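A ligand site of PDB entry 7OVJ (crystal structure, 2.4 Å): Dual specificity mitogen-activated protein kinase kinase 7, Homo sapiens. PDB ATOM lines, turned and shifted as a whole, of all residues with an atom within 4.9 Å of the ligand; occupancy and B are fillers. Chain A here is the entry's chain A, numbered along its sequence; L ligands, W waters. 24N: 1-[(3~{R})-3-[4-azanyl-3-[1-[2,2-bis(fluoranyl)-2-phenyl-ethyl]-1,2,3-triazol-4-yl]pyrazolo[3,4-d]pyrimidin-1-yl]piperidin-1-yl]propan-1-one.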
ATOM      1  N   MET A  36      -6.894  -1.577 -32.808  1.00  0.00           N
ATOM      2  CA  MET A  36      -6.919  -2.301 -31.557  1.00  0.00           C
ATOM      3  C   MET A  36      -7.337  -3.751 -31.815  1.00  0.00           C
ATOM      4  O   MET A  36      -8.322  -3.994 -32.515  1.00  0.00           O
ATOM      5  CB  MET A  36      -7.879  -1.641 -30.564  1.00  0.00           C
ATOM      6  CG  MET A  36      -7.725  -0.134 -30.471  1.00  0.00           C
ATOM      7  SD  MET A  36      -8.767   0.610 -29.207  1.00  0.00           S
ATOM      8  CE  MET A  36      -7.983  -0.018 -27.718  1.00  0.00           C
ATOM      9  N   GLY A  37      -6.577  -4.686 -31.250  1.00  0.00           N
ATOM     10  CA  GLY A  37      -6.914  -6.087 -31.392  1.00  0.00           C
ATOM     11  C   GLY A  37      -6.788  -6.584 -32.832  1.00  0.00           C
ATOM     12  O   GLY A  37      -6.067  -6.034 -33.658  1.00  0.00           O
ATOM     13  N   SER A  38      -7.522  -7.662 -33.108  1.00  0.00           N
ATOM     14  CA  SER A  38      -7.522  -8.281 -34.422  1.00  0.00           C
ATOM     15  C   SER A  38      -8.908  -8.830 -34.707  1.00  0.00           C
ATOM     16  O   SER A  38      -9.789  -8.835 -33.846  1.00  0.00           O
ATOM     17  CB  SER A  38      -6.455  -9.387 -34.531  1.00  0.00           C
ATOM     18  OG  SER A  38      -6.627 -10.350 -33.500  1.00  0.00           O
ATOM     19  N   VAL A  44     -11.726  -1.704 -35.185  1.00  0.00           N
ATOM     20  CA  VAL A  44     -11.845  -0.644 -34.190  1.00  0.00           C
ATOM     21  C   VAL A  44     -10.489   0.029 -34.041  1.00  0.00           C
ATOM     22  O   VAL A  44      -9.508  -0.606 -33.650  1.00  0.00           O
ATOM     23  CB  VAL A  44     -12.344  -1.191 -32.839  1.00  0.00           C
ATOM     24  CG1 VAL A  44     -12.401  -0.082 -31.808  1.00  0.00           C
ATOM     25  CG2 VAL A  44     -13.700  -1.840 -33.005  1.00  0.00           C
ATOM     26  N   ALA A  57     -11.821   5.452 -28.976  1.00  0.00           N
ATOM     27  CA  ALA A  57     -11.994   4.285 -29.824  1.00  0.00           C
ATOM     28  C   ALA A  57     -12.945   4.640 -30.954  1.00  0.00           C
ATOM     29  O   ALA A  57     -13.982   5.262 -30.723  1.00  0.00           O
ATOM     30  CB  ALA A  57     -12.528   3.091 -29.035  1.00  0.00           C
ATOM     31  N   LYS A  59     -14.922   3.051 -34.351  1.00  0.00           N
ATOM     32  CA  LYS A  59     -15.368   1.963 -35.210  1.00  0.00           C
ATOM     33  C   LYS A  59     -15.651   2.516 -36.605  1.00  0.00           C
ATOM     34  O   LYS A  59     -16.399   3.485 -36.753  1.00  0.00           O
ATOM     35  CB  LYS A  59     -16.620   1.300 -34.632  1.00  0.00           C
ATOM     36  CG  LYS A  59     -17.302   0.313 -35.552  1.00  0.00           C
ATOM     37  CD  LYS A  59     -16.620  -1.046 -35.532  1.00  0.00           C
ATOM     38  CE  LYS A  59     -17.433  -2.085 -36.277  1.00  0.00           C
ATOM     39  NZ  LYS A  59     -16.805  -3.428 -36.246  1.00  0.00           N
ATOM     40  N   ILE A  73     -24.281  -3.369 -37.525  1.00  0.00           N
ATOM     41  CA  ILE A  73     -23.607  -2.266 -36.863  1.00  0.00           C
ATOM     42  C   ILE A  73     -24.571  -1.113 -36.627  1.00  0.00           C
ATOM     43  O   ILE A  73     -24.539  -0.457 -35.570  1.00  0.00           O
ATOM     44  CB  ILE A  73     -22.381  -1.811 -37.689  1.00  0.00           C
ATOM     45  CG1 ILE A  73     -21.328  -2.922 -37.718  1.00  0.00           C
ATOM     46  CG2 ILE A  73     -21.799  -0.528 -37.137  1.00  0.00           C
ATOM     47  CD1 ILE A  73     -20.164  -2.622 -38.642  1.00  0.00           C
ATOM     48  N   ASP A  76     -26.939  -1.970 -33.731  1.00  0.00           N
ATOM     49  CA  ASP A  76     -26.207  -1.899 -32.470  1.00  0.00           C
ATOM     50  C   ASP A  76     -25.866  -0.467 -32.103  1.00  0.00           C
ATOM     51  O   ASP A  76     -25.906  -0.087 -30.928  1.00  0.00           O
ATOM     52  CB  ASP A  76     -24.952  -2.757 -32.548  1.00  0.00           C
ATOM     53  CG  ASP A  76     -25.249  -4.237 -32.709  1.00  0.00           C
ATOM     54  OD1 ASP A  76     -26.444  -4.594 -32.758  1.00  0.00           O
ATOM     55  OD2 ASP A  76     -24.302  -5.035 -32.791  1.00  0.00           O
ATOM     56  N   LEU A  77     -25.524   0.353 -33.109  1.00  0.00           N
ATOM     57  CA  LEU A  77     -25.316   1.777 -32.855  1.00  0.00           C
ATOM     58  C   LEU A  77     -26.588   2.428 -32.339  1.00  0.00           C
ATOM     59  O   LEU A  77     -26.536   3.320 -31.484  1.00  0.00           O
ATOM     60  CB  LEU A  77     -24.839   2.472 -34.128  1.00  0.00           C
ATOM     61  CG  LEU A  77     -24.698   3.988 -34.074  1.00  0.00           C
ATOM     62  CD1 LEU A  77     -23.718   4.395 -32.992  1.00  0.00           C
ATOM     63  CD2 LEU A  77     -24.274   4.552 -35.423  1.00  0.00           C
ATOM     64  N   VAL A  80     -26.812   1.680 -28.703  1.00  0.00           N
ATOM     65  CA  VAL A  80     -25.763   2.428 -28.013  1.00  0.00           C
ATOM     66  C   VAL A  80     -26.140   3.900 -27.886  1.00  0.00           C
ATOM     67  O   VAL A  80     -25.965   4.514 -26.823  1.00  0.00           O
ATOM     68  CB  VAL A  80     -24.409   2.248 -28.733  1.00  0.00           C
ATOM     69  CG1 VAL A  80     -23.381   3.242 -28.214  1.00  0.00           C
ATOM     70  CG2 VAL A  80     -23.907   0.826 -28.571  1.00  0.00           C
ATOM     71  N   VAL A  90     -20.782   0.981 -22.654  1.00  0.00           N
ATOM     72  CA  VAL A  90     -19.776   1.830 -23.281  1.00  0.00           C
ATOM     73  C   VAL A  90     -20.463   2.921 -24.089  1.00  0.00           C
ATOM     74  O   VAL A  90     -21.300   2.649 -24.952  1.00  0.00           O
ATOM     75  CB  VAL A  90     -18.839   0.976 -24.156  1.00  0.00           C
ATOM     76  CG1 VAL A  90     -17.814   1.864 -24.839  1.00  0.00           C
ATOM     77  CG2 VAL A  90     -18.165  -0.090 -23.325  1.00  0.00           C
ATOM     78  N   ILE A 104     -17.718   5.703 -35.896  1.00  0.00           N
ATOM     79  CA  ILE A 104     -18.417   5.729 -34.617  1.00  0.00           C
ATOM     80  C   ILE A 104     -17.380   5.905 -33.522  1.00  0.00           C
ATOM     81  O   ILE A 104     -16.510   5.048 -33.340  1.00  0.00           O
ATOM     82  CB  ILE A 104     -19.244   4.455 -34.393  1.00  0.00           C
ATOM     83  CG1 ILE A 104     -20.178   4.219 -35.585  1.00  0.00           C
ATOM     84  CG2 ILE A 104     -20.028   4.560 -33.095  1.00  0.00           C
ATOM     85  CD1 ILE A 104     -20.883   2.881 -35.539  1.00  0.00           C
ATOM     86  N   MET A 106     -16.262   6.032 -29.684  1.00  0.00           N
ATOM     87  CA  MET A 106     -16.631   5.479 -28.393  1.00  0.00           C
ATOM     88  C   MET A 106     -15.575   5.851 -27.355  1.00  0.00           C
ATOM     89  O   MET A 106     -14.428   6.129 -27.688  1.00  0.00           O
ATOM     90  CB  MET A 106     -16.764   3.948 -28.469  1.00  0.00           C
ATOM     91  CG  MET A 106     -17.614   3.446 -29.632  1.00  0.00           C
ATOM     92  SD  MET A 106     -19.385   3.674 -29.371  1.00  0.00           S
ATOM     93  CE  MET A 106     -19.645   2.632 -27.948  1.00  0.00           C
ATOM     94  N   GLU A 107     -15.997   5.861 -26.097  1.00  0.00           N
ATOM     95  CA  GLU A 107     -15.045   6.120 -25.013  1.00  0.00           C
ATOM     96  C   GLU A 107     -14.010   5.013 -24.961  1.00  0.00           C
ATOM     97  O   GLU A 107     -14.329   3.820 -25.077  1.00  0.00           O
ATOM     98  CB  GLU A 107     -15.780   6.233 -23.673  1.00  0.00           C
ATOM     99  CG  GLU A 107     -16.625   5.023 -23.310  1.00  0.00           C
ATOM    100  CD  GLU A 107     -17.257   5.150 -21.938  1.00  0.00           C
ATOM    101  OE1 GLU A 107     -16.696   5.870 -21.082  1.00  0.00           O
ATOM    102  OE2 GLU A 107     -18.319   4.535 -21.716  1.00  0.00           O
ATOM    103  N   LEU A 108     -12.748   5.402 -24.807  1.00  0.00           N
ATOM    104  CA  LEU A 108     -11.650   4.446 -24.816  1.00  0.00           C
ATOM    105  C   LEU A 108     -11.569   3.742 -23.471  1.00  0.00           C
ATOM    106  O   LEU A 108     -11.420   4.391 -22.435  1.00  0.00           O
ATOM    107  CB  LEU A 108     -10.328   5.138 -25.149  1.00  0.00           C
ATOM    108  CG  LEU A 108      -9.131   4.205 -25.307  1.00  0.00           C
ATOM    109  CD1 LEU A 108      -9.378   3.202 -26.427  1.00  0.00           C
ATOM    110  CD2 LEU A 108      -7.853   5.000 -25.566  1.00  0.00           C
ATOM    111  N   MET A 109     -11.674   2.419 -23.481  1.00  0.00           N
ATOM    112  CA  MET A 109     -11.467   1.595 -22.301  1.00  0.00           C
ATOM    113  C   MET A 109     -10.073   0.994 -22.337  1.00  0.00           C
ATOM    114  O   MET A 109      -9.330   1.132 -23.304  1.00  0.00           O
ATOM    115  CB  MET A 109     -12.543   0.505 -22.217  1.00  0.00           C
ATOM    116  CG  MET A 109     -13.972   1.016 -22.324  1.00  0.00           C
ATOM    117  SD  MET A 109     -14.546   1.868 -20.843  1.00  0.00           S
ATOM    118  CE  MET A 109     -14.804   0.482 -19.733  1.00  0.00           C
ATOM    119  N   GLY A 110      -9.708   0.316 -21.249  1.00  0.00           N
ATOM    120  CA  GLY A 110      -8.413  -0.327 -21.170  1.00  0.00           C
ATOM    121  C   GLY A 110      -8.336  -1.599 -21.969  1.00  0.00           C
ATOM    122  O   GLY A 110      -7.660  -1.654 -23.010  1.00  0.00           O
ATOM    123  N   CYS A 112     -10.454  -5.896 -22.209  1.00  0.00           N
ATOM    124  CA  CYS A 112     -11.594  -6.736 -21.844  1.00  0.00           C
ATOM    125  C   CYS A 112     -11.190  -7.742 -20.765  1.00  0.00           C
ATOM    126  O   CYS A 112     -10.011  -7.950 -20.472  1.00  0.00           O
ATOM    127  CB  CYS A 112     -12.135  -7.468 -23.084  1.00  0.00           C
ATOM    128  SG  CYS A 112     -10.931  -8.534 -23.892  1.00  0.00           S
ATOM    129  N   GLU A 114     -11.451 -10.905 -20.909  1.00  0.00           N
ATOM    130  CA  GLU A 114     -10.757 -12.049 -21.508  1.00  0.00           C
ATOM    131  C   GLU A 114      -9.249 -11.822 -21.503  1.00  0.00           C
ATOM    132  O   GLU A 114      -8.475 -12.715 -21.134  1.00  0.00           O
ATOM    133  CB  GLU A 114     -11.270 -12.296 -22.921  1.00  0.00           C
ATOM    134  CG  GLU A 114     -10.319 -13.086 -23.808  1.00  0.00           C
ATOM    135  CD  GLU A 114     -10.800 -13.168 -25.241  1.00  0.00           C
ATOM    136  OE1 GLU A 114     -11.936 -13.621 -25.462  1.00  0.00           O
ATOM    137  OE2 GLU A 114     -10.039 -12.757 -26.144  1.00  0.00           O
ATOM    138  N   LYS A 115      -8.807 -10.628 -21.920  1.00  0.00           N
ATOM    139  CA  LYS A 115      -7.388 -10.331 -21.937  1.00  0.00           C
ATOM    140  C   LYS A 115      -6.844 -10.055 -20.541  1.00  0.00           C
ATOM    141  O   LYS A 115      -5.647 -10.249 -20.297  1.00  0.00           O
ATOM    142  CB  LYS A 115      -7.109  -9.146 -22.870  1.00  0.00           C
ATOM    143  CG  LYS A 115      -7.357  -9.468 -24.331  1.00  0.00           C
ATOM    144  CD  LYS A 115      -6.961  -8.316 -25.246  1.00  0.00           C
ATOM    145  CE  LYS A 115      -7.085  -8.711 -26.705  1.00  0.00           C
ATOM    146  NZ  LYS A 115      -6.756  -7.582 -27.624  1.00  0.00           N
ATOM    147  N   SER A 157     -15.112 -11.337 -23.347  1.00  0.00           N
ATOM    148  CA  SER A 157     -14.626 -10.400 -24.349  1.00  0.00           C
ATOM    149  C   SER A 157     -15.544  -9.196 -24.540  1.00  0.00           C
ATOM    150  O   SER A 157     -15.146  -8.241 -25.207  1.00  0.00           O
ATOM    151  CB  SER A 157     -14.434 -11.111 -25.694  1.00  0.00           C
ATOM    152  OG  SER A 157     -15.640 -11.684 -26.152  1.00  0.00           O
ATOM    153  N   LEU A 160     -15.616  -4.709 -20.570  1.00  0.00           N
ATOM    154  CA  LEU A 160     -14.478  -3.811 -20.666  1.00  0.00           C
ATOM    155  C   LEU A 160     -14.201  -3.146 -19.325  1.00  0.00           C
ATOM    156  O   LEU A 160     -15.116  -2.841 -18.557  1.00  0.00           O
ATOM    157  CB  LEU A 160     -14.694  -2.735 -21.735  1.00  0.00           C
ATOM    158  CG  LEU A 160     -14.997  -3.225 -23.146  1.00  0.00           C
ATOM    159  CD1 LEU A 160     -15.138  -2.046 -24.102  1.00  0.00           C
ATOM    160  CD2 LEU A 160     -13.932  -4.185 -23.641  1.00  0.00           C
ATOM    161  N   CYS A 170     -20.260  -4.029 -23.734  1.00  0.00           N
ATOM    162  CA  CYS A 170     -20.199  -3.586 -25.120  1.00  0.00           C
ATOM    163  C   CYS A 170     -20.510  -4.757 -26.039  1.00  0.00           C
ATOM    164  O   CYS A 170     -20.644  -5.901 -25.595  1.00  0.00           O
ATOM    165  CB  CYS A 170     -18.827  -2.993 -25.454  1.00  0.00           C
ATOM    166  SG  CYS A 170     -17.549  -4.227 -25.769  1.00  0.00           S
ATOM    167  N   ASP A 171     -20.611  -4.453 -27.323  1.00  0.00           N
ATOM    168  CA  ASP A 171     -20.760  -5.434 -28.400  1.00  0.00           C
ATOM    169  C   ASP A 171     -21.921  -6.398 -28.130  1.00  0.00           C
ATOM    170  O   ASP A 171     -21.742  -7.587 -27.870  1.00  0.00           O
ATOM    171  CB  ASP A 171     -19.450  -6.204 -28.608  1.00  0.00           C
ATOM    172  CG  ASP A 171     -18.416  -5.412 -29.393  1.00  0.00           C
ATOM    173  OD1 ASP A 171     -18.826  -4.605 -30.244  1.00  0.00           O
ATOM    174  OD2 ASP A 171     -17.210  -5.601 -29.148  1.00  0.00           O
HETATM  175  C4  24N L   1     -12.171  -1.636 -27.140  1.00  0.00           C
HETATM  176  C5  24N L   1     -13.261  -0.861 -27.091  1.00  0.00           C
HETATM  177  C6  24N L   1     -13.262   0.240 -26.323  1.00  0.00           C
HETATM  178  N1  24N L   1     -12.205   0.604 -25.588  1.00  0.00           N
HETATM  179  N3  24N L   1     -11.073  -1.327 -26.432  1.00  0.00           N
HETATM  180  C2  24N L   1     -11.052  -0.186 -25.628  1.00  0.00           C
HETATM  181  CAI 24N L   1     -14.162  -1.441 -27.902  1.00  0.00           C
HETATM  182  CAK 24N L   1     -15.403  -1.040 -28.182  1.00  0.00           C
HETATM  183  CAL 24N L   1     -11.459  -3.741 -28.289  1.00  0.00           C
HETATM  184  CAM 24N L   1     -11.282  -3.834 -29.790  1.00  0.00           C
HETATM  185  CAN 24N L   1     -10.178  -4.831 -30.087  1.00  0.00           C
HETATM  186  CAO 24N L   1     -10.577  -6.211 -29.622  1.00  0.00           C
HETATM  187  CAQ 24N L   1     -11.938  -5.081 -27.749  1.00  0.00           C
HETATM  188  CAR 24N L   1     -10.786  -7.230 -27.430  1.00  0.00           C
HETATM  189  CAT 24N L   1     -11.347  -7.162 -26.014  1.00  0.00           C
HETATM  190  CAU 24N L   1     -16.218  -1.653 -29.026  1.00  0.00           C
HETATM  191  CAY 24N L   1     -18.566  -1.269 -29.857  1.00  0.00           C
HETATM  192  CAZ 24N L   1     -18.406  -0.663 -31.253  1.00  0.00           C
HETATM  193  CBA 24N L   1     -19.758  -0.636 -31.972  1.00  0.00           C
HETATM  194  CBB 24N L   1     -20.136  -1.709 -32.779  1.00  0.00           C
HETATM  195  CBC 24N L   1     -21.354  -1.690 -33.438  1.00  0.00           C
HETATM  196  CBD 24N L   1     -22.207  -0.593 -33.299  1.00  0.00           C
HETATM  197  CBE 24N L   1     -21.828   0.480 -32.491  1.00  0.00           C
HETATM  198  CBF 24N L   1     -20.606   0.452 -31.834  1.00  0.00           C
HETATM  199  CBI 24N L   1     -11.630  -8.579 -25.513  1.00  0.00           C
HETATM  200  FBG 24N L   1     -17.966   0.579 -31.130  1.00  0.00           F
HETATM  201  FBH 24N L   1     -17.537  -1.381 -31.951  1.00  0.00           F
HETATM  202  NAG 24N L   1     -12.406  -2.659 -27.950  1.00  0.00           N
HETATM  203  NAH 24N L   1     -13.651  -2.539 -28.436  1.00  0.00           N
HETATM  204  NAJ 24N L   1     -14.379   0.983 -26.309  1.00  0.00           N
HETATM  205  NAP 24N L   1     -11.089  -6.195 -28.233  1.00  0.00           N
HETATM  206  NAV 24N L   1     -17.353  -0.959 -29.048  1.00  0.00           N
HETATM  207  NAW 24N L   1     -17.229   0.084 -28.215  1.00  0.00           N
HETATM  208  NAX 24N L   1     -16.002   0.038 -27.671  1.00  0.00           N
HETATM  209  OAS 24N L   1     -10.093  -8.179 -27.784  1.00  0.00           O
HETATM  210  O   HOH W   1     -20.507  -4.813 -34.256  1.00  0.00           O
HETATM  211  O   HOH W   2      -8.253  -3.164 -25.956  1.00  0.00           O
HETATM  212  O   HOH W   3     -21.254  -1.594 -28.147  1.00  0.00           O
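SG of Cys 112 is covalently linked to CBI of the ligand (1.8 Å).
N1 of the ligand is in hydrogen-bond range of N of Met 109 (2.8 Å).
NAJ of the ligand lies within hydrogen-bond range of O of Glu 107 (3.1 Å).
NZ of Lys 115 sits close to OAS of the ligand, at 3.4 Å.
The side-chain sulfur of Cys 112 sits at hydrogen-bond distance from the backbone NH of Lys 115, 3.6 Å away.
The backbone NH (N) of Met 36 is in hydrogen-bond range of the backbone carbonyl oxygen (O) of Val 44, 2.9 Å away.
The backbone carbonyl oxygen (O) of Ala 57 lies within hydrogen-bond range of the backbone NH (N) of Met 106, at 2.6 Å.
The side-chain sulfur of Cys 170 lies within hydrogen-bond range of the side-chain carboxylate of Asp 171, at 3.7 Å.
O of Lys 59 sits at hydrogen-bond distance from N of Ile 104 (2.7 Å).
Merely in contact with the ligand: Met 36, Met 106, Ile 73, Asp 171, Leu 77, Ser 157, Asp 76, Leu 160, Lys 59, Gly 37, Val 90, Leu 108, Ala 57 and Ile 104.
Hydrophobic or aromatic side chains within 4 Å of the ligand: Met 36, Ala 57, Ile 73, Leu 77, Val 90, Ile 104, Met 106, Leu 108, Met 109 and Leu 160.
Water W2 lies within hydrogen-bond range of O of Gly 110 (3.4 Å) and N3 of the ligand (3.4 Å).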
